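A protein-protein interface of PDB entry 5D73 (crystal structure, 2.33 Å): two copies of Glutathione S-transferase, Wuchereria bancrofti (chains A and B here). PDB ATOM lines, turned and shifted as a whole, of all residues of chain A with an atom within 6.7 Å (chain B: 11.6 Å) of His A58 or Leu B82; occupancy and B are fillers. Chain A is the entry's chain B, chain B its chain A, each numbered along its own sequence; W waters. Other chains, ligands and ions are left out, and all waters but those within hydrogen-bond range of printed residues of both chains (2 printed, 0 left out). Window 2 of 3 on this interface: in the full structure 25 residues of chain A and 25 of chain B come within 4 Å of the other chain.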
ATOM      1  N   CYS A  52      31.751  25.247  -1.169  1.00  0.00           N
ATOM      2  CA  CYS A  52      30.718  26.251  -0.992  1.00  0.00           C
ATOM      3  C   CYS A  52      30.498  27.032  -2.275  1.00  0.00           C
ATOM      4  O   CYS A  52      31.452  27.409  -2.932  1.00  0.00           O
ATOM      5  CB  CYS A  52      31.086  27.232   0.133  1.00  0.00           C
ATOM      6  SG  CYS A  52      29.881  28.563   0.274  1.00  0.00           S
ATOM      7  N   LEU A  53      29.237  27.258  -2.612  1.00  0.00           N
ATOM      8  CA  LEU A  53      28.838  28.097  -3.723  1.00  0.00           C
ATOM      9  C   LEU A  53      27.944  29.249  -3.248  1.00  0.00           C
ATOM     10  O   LEU A  53      26.843  29.026  -2.727  1.00  0.00           O
ATOM     11  CB  LEU A  53      28.081  27.291  -4.802  1.00  0.00           C
ATOM     12  CG  LEU A  53      27.652  28.090  -6.069  1.00  0.00           C
ATOM     13  CD1 LEU A  53      28.843  28.304  -7.001  1.00  0.00           C
ATOM     14  CD2 LEU A  53      26.518  27.401  -6.823  1.00  0.00           C
ATOM     15  N   TYR A  54      28.405  30.472  -3.466  1.00  0.00           N
ATOM     16  CA  TYR A  54      27.571  31.622  -3.238  1.00  0.00           C
ATOM     17  C   TYR A  54      26.879  31.931  -4.561  1.00  0.00           C
ATOM     18  O   TYR A  54      27.520  32.141  -5.575  1.00  0.00           O
ATOM     19  CB  TYR A  54      28.355  32.815  -2.633  1.00  0.00           C
ATOM     20  CG  TYR A  54      28.391  32.857  -1.099  1.00  0.00           C
ATOM     21  CD1 TYR A  54      27.377  33.489  -0.371  1.00  0.00           C
ATOM     22  CD2 TYR A  54      29.430  32.274  -0.385  1.00  0.00           C
ATOM     23  CE1 TYR A  54      27.389  33.527   1.038  1.00  0.00           C
ATOM     24  CE2 TYR A  54      29.460  32.300   1.022  1.00  0.00           C
ATOM     25  CZ  TYR A  54      28.441  32.932   1.740  1.00  0.00           C
ATOM     26  OH  TYR A  54      28.496  32.974   3.146  1.00  0.00           O
ATOM     27  N   ASP A  55      25.560  31.882  -4.551  1.00  0.00           N
ATOM     28  CA  ASP A  55      24.726  32.295  -5.660  1.00  0.00           C
ATOM     29  C   ASP A  55      24.114  33.595  -5.157  1.00  0.00           C
ATOM     30  O   ASP A  55      23.236  33.591  -4.299  1.00  0.00           O
ATOM     31  CB  ASP A  55      23.670  31.227  -5.908  1.00  0.00           C
ATOM     32  CG  ASP A  55      22.669  31.589  -6.981  1.00  0.00           C
ATOM     33  OD1 ASP A  55      22.647  32.752  -7.438  1.00  0.00           O
ATOM     34  OD2 ASP A  55      21.863  30.701  -7.357  1.00  0.00           O
ATOM     35  N   GLY A  56      24.596  34.718  -5.697  1.00  0.00           N
ATOM     36  CA  GLY A  56      24.343  36.030  -5.107  1.00  0.00           C
ATOM     37  C   GLY A  56      24.857  36.024  -3.679  1.00  0.00           C
ATOM     38  O   GLY A  56      26.017  35.720  -3.453  1.00  0.00           O
ATOM     39  N   ASP A  57      23.953  36.311  -2.741  1.00  0.00           N
ATOM     40  CA  ASP A  57      24.204  36.304  -1.297  1.00  0.00           C
ATOM     41  C   ASP A  57      23.934  34.965  -0.599  1.00  0.00           C
ATOM     42  O   ASP A  57      24.209  34.834   0.592  1.00  0.00           O
ATOM     43  CB  ASP A  57      23.305  37.348  -0.621  1.00  0.00           C
ATOM     44  CG  ASP A  57      23.717  38.753  -0.930  1.00  0.00           C
ATOM     45  OD1 ASP A  57      24.896  38.960  -1.305  1.00  0.00           O
ATOM     46  OD2 ASP A  57      22.861  39.655  -0.756  1.00  0.00           O
ATOM     47  N   HIS A  58      23.401  33.989  -1.324  1.00  0.00           N
ATOM     48  CA  HIS A  58      22.960  32.723  -0.729  1.00  0.00           C
ATOM     49  C   HIS A  58      24.097  31.726  -0.625  1.00  0.00           C
ATOM     50  O   HIS A  58      24.680  31.334  -1.640  1.00  0.00           O
ATOM     51  CB  HIS A  58      21.804  32.135  -1.533  1.00  0.00           C
ATOM     52  CG  HIS A  58      20.697  33.111  -1.768  1.00  0.00           C
ATOM     53  ND1 HIS A  58      19.910  33.600  -0.743  1.00  0.00           N
ATOM     54  CD2 HIS A  58      20.271  33.727  -2.899  1.00  0.00           C
ATOM     55  CE1 HIS A  58      19.032  34.455  -1.239  1.00  0.00           C
ATOM     56  NE2 HIS A  58      19.231  34.552  -2.543  1.00  0.00           N
ATOM     57  N   GLN A  59      24.418  31.317   0.608  1.00  0.00           N
ATOM     58  CA  GLN A  59      25.468  30.319   0.852  1.00  0.00           C
ATOM     59  C   GLN A  59      24.943  28.903   0.595  1.00  0.00           C
ATOM     60  O   GLN A  59      23.991  28.476   1.230  1.00  0.00           O
ATOM     61  CB  GLN A  59      25.967  30.418   2.291  1.00  0.00           C
ATOM     62  CG  GLN A  59      27.106  29.461   2.598  1.00  0.00           C
ATOM     63  CD  GLN A  59      27.419  29.325   4.075  1.00  0.00           C
ATOM     64  OE1 GLN A  59      27.845  28.258   4.527  1.00  0.00           O
ATOM     65  NE2 GLN A  59      27.239  30.395   4.831  1.00  0.00           N
ATOM     66  N   ILE A  60      25.576  28.169  -0.319  1.00  0.00           N
ATOM     67  CA  ILE A  60      25.182  26.771  -0.571  1.00  0.00           C
ATOM     68  C   ILE A  60      26.375  25.845  -0.384  1.00  0.00           C
ATOM     69  O   ILE A  60      27.313  25.794  -1.245  1.00  0.00           O
ATOM     70  CB  ILE A  60      24.525  26.540  -1.945  1.00  0.00           C
ATOM     71  CG1 ILE A  60      23.354  27.515  -2.172  1.00  0.00           C
ATOM     72  CG2 ILE A  60      23.982  25.115  -2.009  1.00  0.00           C
ATOM     73  CD1 ILE A  60      22.808  27.563  -3.607  1.00  0.00           C
ATOM     74  N   HIS A  69      20.852  21.994  -7.112  1.00  0.00           N
ATOM     75  CA  HIS A  69      20.476  23.408  -7.240  1.00  0.00           C
ATOM     76  C   HIS A  69      20.794  23.937  -8.677  1.00  0.00           C
ATOM     77  O   HIS A  69      19.936  24.485  -9.357  1.00  0.00           O
ATOM     78  CB  HIS A  69      21.191  24.282  -6.194  1.00  0.00           C
ATOM     79  CG  HIS A  69      21.036  25.758  -6.445  1.00  0.00           C
ATOM     80  ND1 HIS A  69      19.829  26.406  -6.364  1.00  0.00           N
ATOM     81  CD2 HIS A  69      21.941  26.707  -6.781  1.00  0.00           C
ATOM     82  CE1 HIS A  69      19.990  27.690  -6.628  1.00  0.00           C
ATOM     83  NE2 HIS A  69      21.269  27.904  -6.870  1.00  0.00           N
ATOM     84  N   ARG A  72      18.405  22.406 -11.403  1.00  0.00           N
ATOM     85  CA  ARG A  72      17.081  23.024 -11.523  1.00  0.00           C
ATOM     86  C   ARG A  72      17.185  24.396 -12.161  1.00  0.00           C
ATOM     87  O   ARG A  72      16.434  24.710 -13.059  1.00  0.00           O
ATOM     88  CB  ARG A  72      16.380  23.114 -10.167  1.00  0.00           C
ATOM     89  CG  ARG A  72      15.963  21.756  -9.610  1.00  0.00           C
ATOM     90  CD  ARG A  72      15.207  21.906  -8.316  1.00  0.00           C
ATOM     91  NE  ARG A  72      16.014  22.563  -7.288  1.00  0.00           N
ATOM     92  CZ  ARG A  72      16.804  21.968  -6.391  1.00  0.00           C
ATOM     93  NH1 ARG A  72      16.937  20.650  -6.331  1.00  0.00           N
ATOM     94  NH2 ARG A  72      17.438  22.713  -5.493  1.00  0.00           N
ATOM     95  N   LEU B  76       6.461  17.834  -0.137  1.00  0.00           N
ATOM     96  CA  LEU B  76       7.289  17.929   1.043  1.00  0.00           C
ATOM     97  C   LEU B  76       8.680  18.379   0.645  1.00  0.00           C
ATOM     98  O   LEU B  76       9.692  17.992   1.292  1.00  0.00           O
ATOM     99  CB  LEU B  76       7.353  16.580   1.779  1.00  0.00           C
ATOM    100  CG  LEU B  76       6.028  16.114   2.343  1.00  0.00           C
ATOM    101  CD1 LEU B  76       6.116  14.669   2.758  1.00  0.00           C
ATOM    102  CD2 LEU B  76       5.552  16.992   3.501  1.00  0.00           C
ATOM    103  N   ASN B  77       8.751  19.216  -0.392  1.00  0.00           N
ATOM    104  CA  ASN B  77      10.030  19.635  -0.976  1.00  0.00           C
ATOM    105  C   ASN B  77      10.283  21.133  -0.880  1.00  0.00           C
ATOM    106  O   ASN B  77      11.165  21.665  -1.557  1.00  0.00           O
ATOM    107  CB  ASN B  77      10.110  19.150  -2.450  1.00  0.00           C
ATOM    108  CG  ASN B  77      11.564  19.045  -3.004  1.00  0.00           C
ATOM    109  OD1 ASN B  77      11.813  19.321  -4.176  1.00  0.00           O
ATOM    110  ND2 ASN B  77      12.488  18.625  -2.193  1.00  0.00           N
ATOM    111  N   GLY B  78       9.518  21.820  -0.030  1.00  0.00           N
ATOM    112  CA  GLY B  78       9.644  23.285   0.173  1.00  0.00           C
ATOM    113  C   GLY B  78       8.745  24.070  -0.753  1.00  0.00           C
ATOM    114  O   GLY B  78       8.103  23.498  -1.632  1.00  0.00           O
ATOM    115  N   GLY B  79       8.689  25.381  -0.557  1.00  0.00           N
ATOM    116  CA  GLY B  79       7.818  26.254  -1.373  1.00  0.00           C
ATOM    117  C   GLY B  79       8.443  26.993  -2.556  1.00  0.00           C
ATOM    118  O   GLY B  79       7.756  27.659  -3.288  1.00  0.00           O
ATOM    119  N   ASN B  80       9.752  26.894  -2.727  1.00  0.00           N
ATOM    120  CA  ASN B  80      10.483  27.568  -3.813  1.00  0.00           C
ATOM    121  C   ASN B  80      11.912  27.031  -3.895  1.00  0.00           C
ATOM    122  O   ASN B  80      12.354  26.291  -3.013  1.00  0.00           O
ATOM    123  CB  ASN B  80      10.502  29.088  -3.599  1.00  0.00           C
ATOM    124  CG  ASN B  80      11.056  29.465  -2.232  1.00  0.00           C
ATOM    125  OD1 ASN B  80      12.116  28.973  -1.828  1.00  0.00           O
ATOM    126  ND2 ASN B  80      10.339  30.302  -1.505  1.00  0.00           N
ATOM    127  N   GLU B  81      12.609  27.403  -4.964  1.00  0.00           N
ATOM    128  CA  GLU B  81      13.990  26.990  -5.213  1.00  0.00           C
ATOM    129  C   GLU B  81      14.897  27.039  -4.006  1.00  0.00           C
ATOM    130  O   GLU B  81      15.601  26.080  -3.732  1.00  0.00           O
ATOM    131  CB  GLU B  81      14.651  27.864  -6.300  1.00  0.00           C
ATOM    132  CG  GLU B  81      16.109  27.479  -6.667  1.00  0.00           C
ATOM    133  CD  GLU B  81      16.241  25.987  -6.962  1.00  0.00           C
ATOM    134  OE1 GLU B  81      15.300  25.426  -7.581  1.00  0.00           O
ATOM    135  OE2 GLU B  81      17.233  25.329  -6.534  1.00  0.00           O
ATOM    136  N   LEU B  82      14.896  28.173  -3.308  1.00  0.00           N
ATOM    137  CA  LEU B  82      15.781  28.389  -2.144  1.00  0.00           C
ATOM    138  C   LEU B  82      15.457  27.474  -0.957  1.00  0.00           C
ATOM    139  O   LEU B  82      16.361  26.999  -0.265  1.00  0.00           O
ATOM    140  CB  LEU B  82      15.697  29.840  -1.678  1.00  0.00           C
ATOM    141  CG  LEU B  82      16.133  30.891  -2.708  1.00  0.00           C
ATOM    142  CD1 LEU B  82      15.846  32.318  -2.235  1.00  0.00           C
ATOM    143  CD2 LEU B  82      17.619  30.710  -3.038  1.00  0.00           C
ATOM    144  N   GLU B  83      14.171  27.247  -0.710  1.00  0.00           N
ATOM    145  CA  GLU B  83      13.767  26.328   0.353  1.00  0.00           C
ATOM    146  C   GLU B  83      14.146  24.870   0.049  1.00  0.00           C
ATOM    147  O   GLU B  83      14.614  24.165   0.925  1.00  0.00           O
ATOM    148  CB  GLU B  83      12.272  26.463   0.610  1.00  0.00           C
ATOM    149  CG  GLU B  83      11.887  27.791   1.283  1.00  0.00           C
ATOM    150  CD  GLU B  83      10.494  27.770   1.847  1.00  0.00           C
ATOM    151  OE1 GLU B  83       9.699  26.916   1.451  1.00  0.00           O
ATOM    152  OE2 GLU B  83      10.184  28.619   2.699  1.00  0.00           O
ATOM    153  N   THR B  84      13.940  24.451  -1.210  1.00  0.00           N
ATOM    154  CA  THR B  84      14.301  23.108  -1.698  1.00  0.00           C
ATOM    155  C   THR B  84      15.783  22.899  -1.495  1.00  0.00           C
ATOM    156  O   THR B  84      16.193  21.924  -0.873  1.00  0.00           O
ATOM    157  CB  THR B  84      13.975  22.975  -3.190  1.00  0.00           C
ATOM    158  OG1 THR B  84      12.585  23.280  -3.425  1.00  0.00           O
ATOM    159  CG2 THR B  84      14.311  21.570  -3.734  1.00  0.00           C
ATOM    160  N   THR B  85      16.595  23.849  -1.976  1.00  0.00           N
ATOM    161  CA  THR B  85      18.035  23.841  -1.750  1.00  0.00           C
ATOM    162  C   THR B  85      18.418  23.773  -0.242  1.00  0.00           C
ATOM    163  O   THR B  85      19.320  23.008   0.141  1.00  0.00           O
ATOM    164  CB  THR B  85      18.680  25.048  -2.460  1.00  0.00           C
ATOM    165  OG1 THR B  85      18.325  25.018  -3.865  1.00  0.00           O
ATOM    166  CG2 THR B  85      20.227  25.074  -2.255  1.00  0.00           C
ATOM    167  N   HIS B  86      17.734  24.573   0.595  1.00  0.00           N
ATOM    168  CA  HIS B  86      17.981  24.610   2.047  1.00  0.00           C
ATOM    169  C   HIS B  86      17.785  23.243   2.710  1.00  0.00           C
ATOM    170  O   HIS B  86      18.616  22.809   3.477  1.00  0.00           O
ATOM    171  CB  HIS B  86      17.056  25.630   2.750  1.00  0.00           C
ATOM    172  CG  HIS B  86      17.424  25.894   4.185  1.00  0.00           C
ATOM    173  ND1 HIS B  86      16.807  25.259   5.238  1.00  0.00           N
ATOM    174  CD2 HIS B  86      18.364  26.698   4.734  1.00  0.00           C
ATOM    175  CE1 HIS B  86      17.341  25.675   6.371  1.00  0.00           C
ATOM    176  NE2 HIS B  86      18.291  26.545   6.092  1.00  0.00           N
ATOM    177  N   ILE B  87      16.669  22.591   2.405  1.00  0.00           N
ATOM    178  CA  ILE B  87      16.342  21.283   2.986  1.00  0.00           C
ATOM    179  C   ILE B  87      17.303  20.179   2.530  1.00  0.00           C
ATOM    180  O   ILE B  87      17.714  19.328   3.342  1.00  0.00           O
ATOM    181  CB  ILE B  87      14.835  20.897   2.823  1.00  0.00           C
ATOM    182  CG1 ILE B  87      14.372  20.818   1.380  1.00  0.00           C
ATOM    183  CG2 ILE B  87      13.968  21.891   3.584  1.00  0.00           C
ATOM    184  CD1 ILE B  87      12.913  20.431   1.204  1.00  0.00           C
ATOM    185  N   ASP B  88      17.719  20.234   1.270  1.00  0.00           N
ATOM    186  CA  ASP B  88      18.714  19.286   0.744  1.00  0.00           C
ATOM    187  C   ASP B  88      20.091  19.423   1.450  1.00  0.00           C
ATOM    188  O   ASP B  88      20.734  18.448   1.824  1.00  0.00           O
ATOM    189  CB  ASP B  88      18.862  19.485  -0.762  1.00  0.00           C
ATOM    190  CG  ASP B  88      19.569  18.341  -1.454  1.00  0.00           C
ATOM    191  OD1 ASP B  88      20.061  17.333  -0.865  1.00  0.00           O
ATOM    192  OD2 ASP B  88      19.629  18.460  -2.671  1.00  0.00           O
ATOM    193  N   MET B  89      20.506  20.655   1.617  1.00  0.00           N
ATOM    194  CA  MET B  89      21.730  20.996   2.340  1.00  0.00           C
ATOM    195  C   MET B  89      21.672  20.470   3.795  1.00  0.00           C
ATOM    196  O   MET B  89      22.591  19.817   4.260  1.00  0.00           O
ATOM    197  CB  MET B  89      21.889  22.513   2.201  1.00  0.00           C
ATOM    198  CG  MET B  89      23.104  23.164   2.755  1.00  0.00           C
ATOM    199  SD  MET B  89      23.174  24.878   2.199  1.00  0.00           S
ATOM    200  CE  MET B  89      22.011  25.630   3.339  1.00  0.00           C
ATOM    201  N   PHE B  90      20.546  20.645   4.464  1.00  0.00           N
ATOM    202  CA  PHE B  90      20.393  20.175   5.846  1.00  0.00           C
ATOM    203  C   PHE B  90      20.382  18.651   5.844  1.00  0.00           C
ATOM    204  O   PHE B  90      21.052  18.024   6.690  1.00  0.00           O
ATOM    205  CB  PHE B  90      19.068  20.690   6.463  1.00  0.00           C
ATOM    206  CG  PHE B  90      19.107  20.946   7.967  1.00  0.00           C
ATOM    207  CD1 PHE B  90      18.514  22.099   8.498  1.00  0.00           C
ATOM    208  CD2 PHE B  90      19.716  20.062   8.843  1.00  0.00           C
ATOM    209  CE1 PHE B  90      18.535  22.359   9.879  1.00  0.00           C
ATOM    210  CE2 PHE B  90      19.757  20.328  10.213  1.00  0.00           C
ATOM    211  CZ  PHE B  90      19.153  21.471  10.738  1.00  0.00           C
ATOM    212  N   CYS B  91      19.633  18.071   4.888  1.00  0.00           N
ATOM    213  CA  CYS B  91      19.550  16.603   4.712  1.00  0.00           C
ATOM    214  C   CYS B  91      20.920  15.943   4.543  1.00  0.00           C
ATOM    215  O   CYS B  91      21.244  15.000   5.257  1.00  0.00           O
ATOM    216  CB  CYS B  91      18.617  16.202   3.567  1.00  0.00           C
ATOM    217  SG  CYS B  91      18.137  14.446   3.574  1.00  0.00           S
ATOM    218  N   LEU B 131      21.631  26.093  12.459  1.00  0.00           N
ATOM    219  CA  LEU B 131      20.920  26.130  11.199  1.00  0.00           C
ATOM    220  C   LEU B 131      19.393  26.123  11.430  1.00  0.00           C
ATOM    221  O   LEU B 131      18.667  26.938  10.854  1.00  0.00           O
ATOM    222  CB  LEU B 131      21.393  24.966  10.324  1.00  0.00           C
ATOM    223  CG  LEU B 131      21.194  25.049   8.816  1.00  0.00           C
ATOM    224  CD1 LEU B 131      21.658  26.366   8.223  1.00  0.00           C
ATOM    225  CD2 LEU B 131      21.897  23.894   8.115  1.00  0.00           C
ATOM    226  N   THR B 134      17.611  29.550  12.180  1.00  0.00           N
ATOM    227  CA  THR B 134      17.414  30.537  11.107  1.00  0.00           C
ATOM    228  C   THR B 134      15.968  30.596  10.556  1.00  0.00           C
ATOM    229  O   THR B 134      15.653  31.462   9.740  1.00  0.00           O
ATOM    230  CB  THR B 134      18.359  30.282   9.914  1.00  0.00           C
ATOM    231  OG1 THR B 134      17.983  29.072   9.249  1.00  0.00           O
ATOM    232  CG2 THR B 134      19.881  30.239  10.364  1.00  0.00           C
ATOM    233  N   ARG B 135      15.099  29.684  10.987  1.00  0.00           N
ATOM    234  CA  ARG B 135      13.696  29.701  10.586  1.00  0.00           C
ATOM    235  C   ARG B 135      12.767  29.636  11.778  1.00  0.00           C
ATOM    236  O   ARG B 135      12.871  28.737  12.603  1.00  0.00           O
ATOM    237  CB  ARG B 135      13.389  28.517   9.671  1.00  0.00           C
ATOM    238  CG  ARG B 135      14.247  28.474   8.417  1.00  0.00           C
ATOM    239  CD  ARG B 135      13.965  29.631   7.502  1.00  0.00           C
ATOM    240  NE  ARG B 135      14.991  29.673   6.451  1.00  0.00           N
ATOM    241  CZ  ARG B 135      14.858  29.222   5.189  1.00  0.00           C
ATOM    242  NH1 ARG B 135      13.721  28.670   4.752  1.00  0.00           N
ATOM    243  NH2 ARG B 135      15.886  29.336   4.339  1.00  0.00           N
ATOM    244  N   ILE B 142      12.114  22.623  10.024  1.00  0.00           N
ATOM    245  CA  ILE B 142      13.331  23.128   9.396  1.00  0.00           C
ATOM    246  C   ILE B 142      13.064  24.372   8.543  1.00  0.00           C
ATOM    247  O   ILE B 142      13.879  25.315   8.564  1.00  0.00           O
ATOM    248  CB  ILE B 142      14.076  22.002   8.614  1.00  0.00           C
ATOM    249  CG1 ILE B 142      14.826  21.118   9.617  1.00  0.00           C
ATOM    250  CG2 ILE B 142      15.073  22.583   7.646  1.00  0.00           C
ATOM    251  CD1 ILE B 142      15.381  19.786   9.126  1.00  0.00           C
ATOM    252  N   LEU B 143      11.939  24.373   7.821  1.00  0.00           N
ATOM    253  CA  LEU B 143      11.542  25.523   7.017  1.00  0.00           C
ATOM    254  C   LEU B 143      10.640  26.538   7.744  1.00  0.00           C
ATOM    255  O   LEU B 143      10.183  27.497   7.154  1.00  0.00           O
ATOM    256  CB  LEU B 143      10.874  25.052   5.733  1.00  0.00           C
ATOM    257  CG  LEU B 143      11.805  24.388   4.730  1.00  0.00           C
ATOM    258  CD1 LEU B 143      10.984  23.860   3.551  1.00  0.00           C
ATOM    259  CD2 LEU B 143      12.844  25.401   4.246  1.00  0.00           C
ATOM    260  N   GLY B 144      10.438  26.347   9.032  1.00  0.00           N
ATOM    261  CA  GLY B 144       9.537  27.169   9.813  1.00  0.00           C
ATOM    262  C   GLY B 144       8.153  26.573   9.751  1.00  0.00           C
ATOM    263  O   GLY B 144       7.915  25.446  10.222  1.00  0.00           O
ATOM    264  N   SER B 148       8.609  19.225   5.850  1.00  0.00           N
ATOM    265  CA  SER B 148       9.253  18.790   4.618  1.00  0.00           C
ATOM    266  C   SER B 148       9.961  17.488   4.868  1.00  0.00           C
ATOM    267  O   SER B 148      10.119  17.056   6.031  1.00  0.00           O
ATOM    268  CB  SER B 148      10.234  19.858   4.112  1.00  0.00           C
ATOM    269  OG  SER B 148      11.299  20.042   5.010  1.00  0.00           O
ATOM    270  N   TYR B 149      10.371  16.820   3.812  1.00  0.00           N
ATOM    271  CA  TYR B 149      10.940  15.479   3.994  1.00  0.00           C
ATOM    272  C   TYR B 149      12.096  15.465   4.980  1.00  0.00           C
ATOM    273  O   TYR B 149      12.216  14.513   5.757  1.00  0.00           O
ATOM    274  CB  TYR B 149      11.354  14.808   2.668  1.00  0.00           C
ATOM    275  CG  TYR B 149      12.626  15.363   1.999  1.00  0.00           C
ATOM    276  CD1 TYR B 149      12.581  16.509   1.219  1.00  0.00           C
ATOM    277  CD2 TYR B 149      13.866  14.703   2.123  1.00  0.00           C
ATOM    278  CE1 TYR B 149      13.724  17.023   0.617  1.00  0.00           C
ATOM    279  CE2 TYR B 149      15.026  15.216   1.519  1.00  0.00           C
ATOM    280  CZ  TYR B 149      14.935  16.380   0.772  1.00  0.00           C
ATOM    281  OH  TYR B 149      16.036  16.888   0.098  1.00  0.00           O
ATOM    282  N   VAL B 150      12.915  16.513   4.975  1.00  0.00           N
ATOM    283  CA  VAL B 150      14.119  16.534   5.797  1.00  0.00           C
ATOM    284  C   VAL B 150      13.817  16.552   7.297  1.00  0.00           C
ATOM    285  O   VAL B 150      14.661  16.128   8.089  1.00  0.00           O
ATOM    286  CB  VAL B 150      15.111  17.659   5.388  1.00  0.00           C
ATOM    287  CG1 VAL B 150      14.532  19.044   5.639  1.00  0.00           C
ATOM    288  CG2 VAL B 150      16.429  17.523   6.132  1.00  0.00           C
HETATM  289  O   HOH W   1      19.765  21.510  -3.673  1.00  0.00           O
HETATM  290  O   HOH W   2      17.322  18.875  -3.938  1.00  0.00           O
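The backbone carbonyl oxygen of Ile A60 is in hydrogen-bond range of the backbone NH of Leu A53 (2.8 Å). O of Asn B77 is in hydrogen-bond range of OG1 of Thr B84, at 2.8 Å. The side-chain amide oxygen (OD1) of Asn B80 lies close to the backbone NH (N) of Leu B82 (3.2 Å). The side-chain carboxylate (OE2) of Glu B81 sits at hydrogen-bond distance from the side-chain hydroxyl (OG1) of Thr B85, 2.9 Å away. The side-chain hydroxyl (OH) of Tyr A54 lies within hydrogen-bond range of the side-chain amide nitrogen (NE2) of Gln A59 (3.3 Å). The side-chain carboxylate of Asp A55 lies within hydrogen-bond range of a ring nitrogen (NE2) of His A69 (2.9 Å).
The side-chain carboxylate (OE2) of Glu B81 lies within salt-bridge range of the guanidinium group (NH2) of Arg A72, 2.8 Å away. A ring nitrogen (ND1) of His A69 is in hydrogen-bond range of the side-chain carboxylate (OE2) of Glu B81, 2.8 Å away. A ring nitrogen (ND1) of His A69 lies within hydrogen-bond range of the side-chain hydroxyl (OG1) of Thr B85 (3.2 Å). The side-chain hydroxyl of Thr B85 is in hydrogen-bond range of the guanidinium group of Arg A72, 3.0 Å away.
No position is printed for both chains. Of the 9 pairs that touch across the chains among the printed residues, none has its exchanged pair printed and touching as well.
His A58 touches Leu B82. Gln A59 touches Met B89 (O to SD, 3.8 Å). CG2 of Ile A60 touches CG2 of Thr B85, at 3.8 Å. CA of Ile A60 touches SD of Met B89, at 3.9 Å. Arg A72 touches Thr B84.
Water W2 lies within hydrogen-bond range of OD2 of Asp B88 and NH1 of Arg A72. Water W1 lies within hydrogen-bond range of NH2 of Arg A72 (3.2 Å) and OD2 of Asp B88 (3.2 Å).
His A58 touches one residue of chain B. No residue of chain B comes within 4 Å of Leu A53. No residue of chain B comes within 4 Å of Asp A55. No residue of chain B comes within 4 Å of Gly A56. Of chain B, only Met B89 (3.8 Å) comes within 4 Å of Gln A59. Printed residues of chain B within 4 Å of His A69: Glu B81 and Thr B85. Of the printed residues of chain A, Thr B84 touches Arg A72 (3.7 Å). Printed residues of chain A within 4 Å of Thr B85: Ile A60 (3.8 Å), His A69 (3.2 Å) and Arg A72 (3.0 Å). Printed residues of chain A within 4 Å of Glu B81: His A69 and Arg A72. Leu B143 touches none of the printed residues of chain A. Thr B134 touches none of the printed residues of chain A. The nearest residue of chain A that does not touch Leu B82 is His A69 (5.3 Å).
Printed residues of chain B that touch a printed residue of chain A: Glu B81, Leu B82, Thr B84, Thr B85 and Met B89. Hydrophobic or aromatic side chains of chain B that line the printed part of chain A: Leu B82 and Met B89. Of the 11 printed residues of chain A, 5 touch a printed residue of chain B. Hydrophobic or aromatic side chains of chain A that line the printed part of chain B: His A58, Ile A60 and His A69. Among the printed residues, 9 pairs touch across the chains. Among the printed residues, Asp or Glu carboxylates within 4 Å of a Lys or Arg side-chain nitrogen of the other chain: Arg A72 with Glu B81 (2.8 Å).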
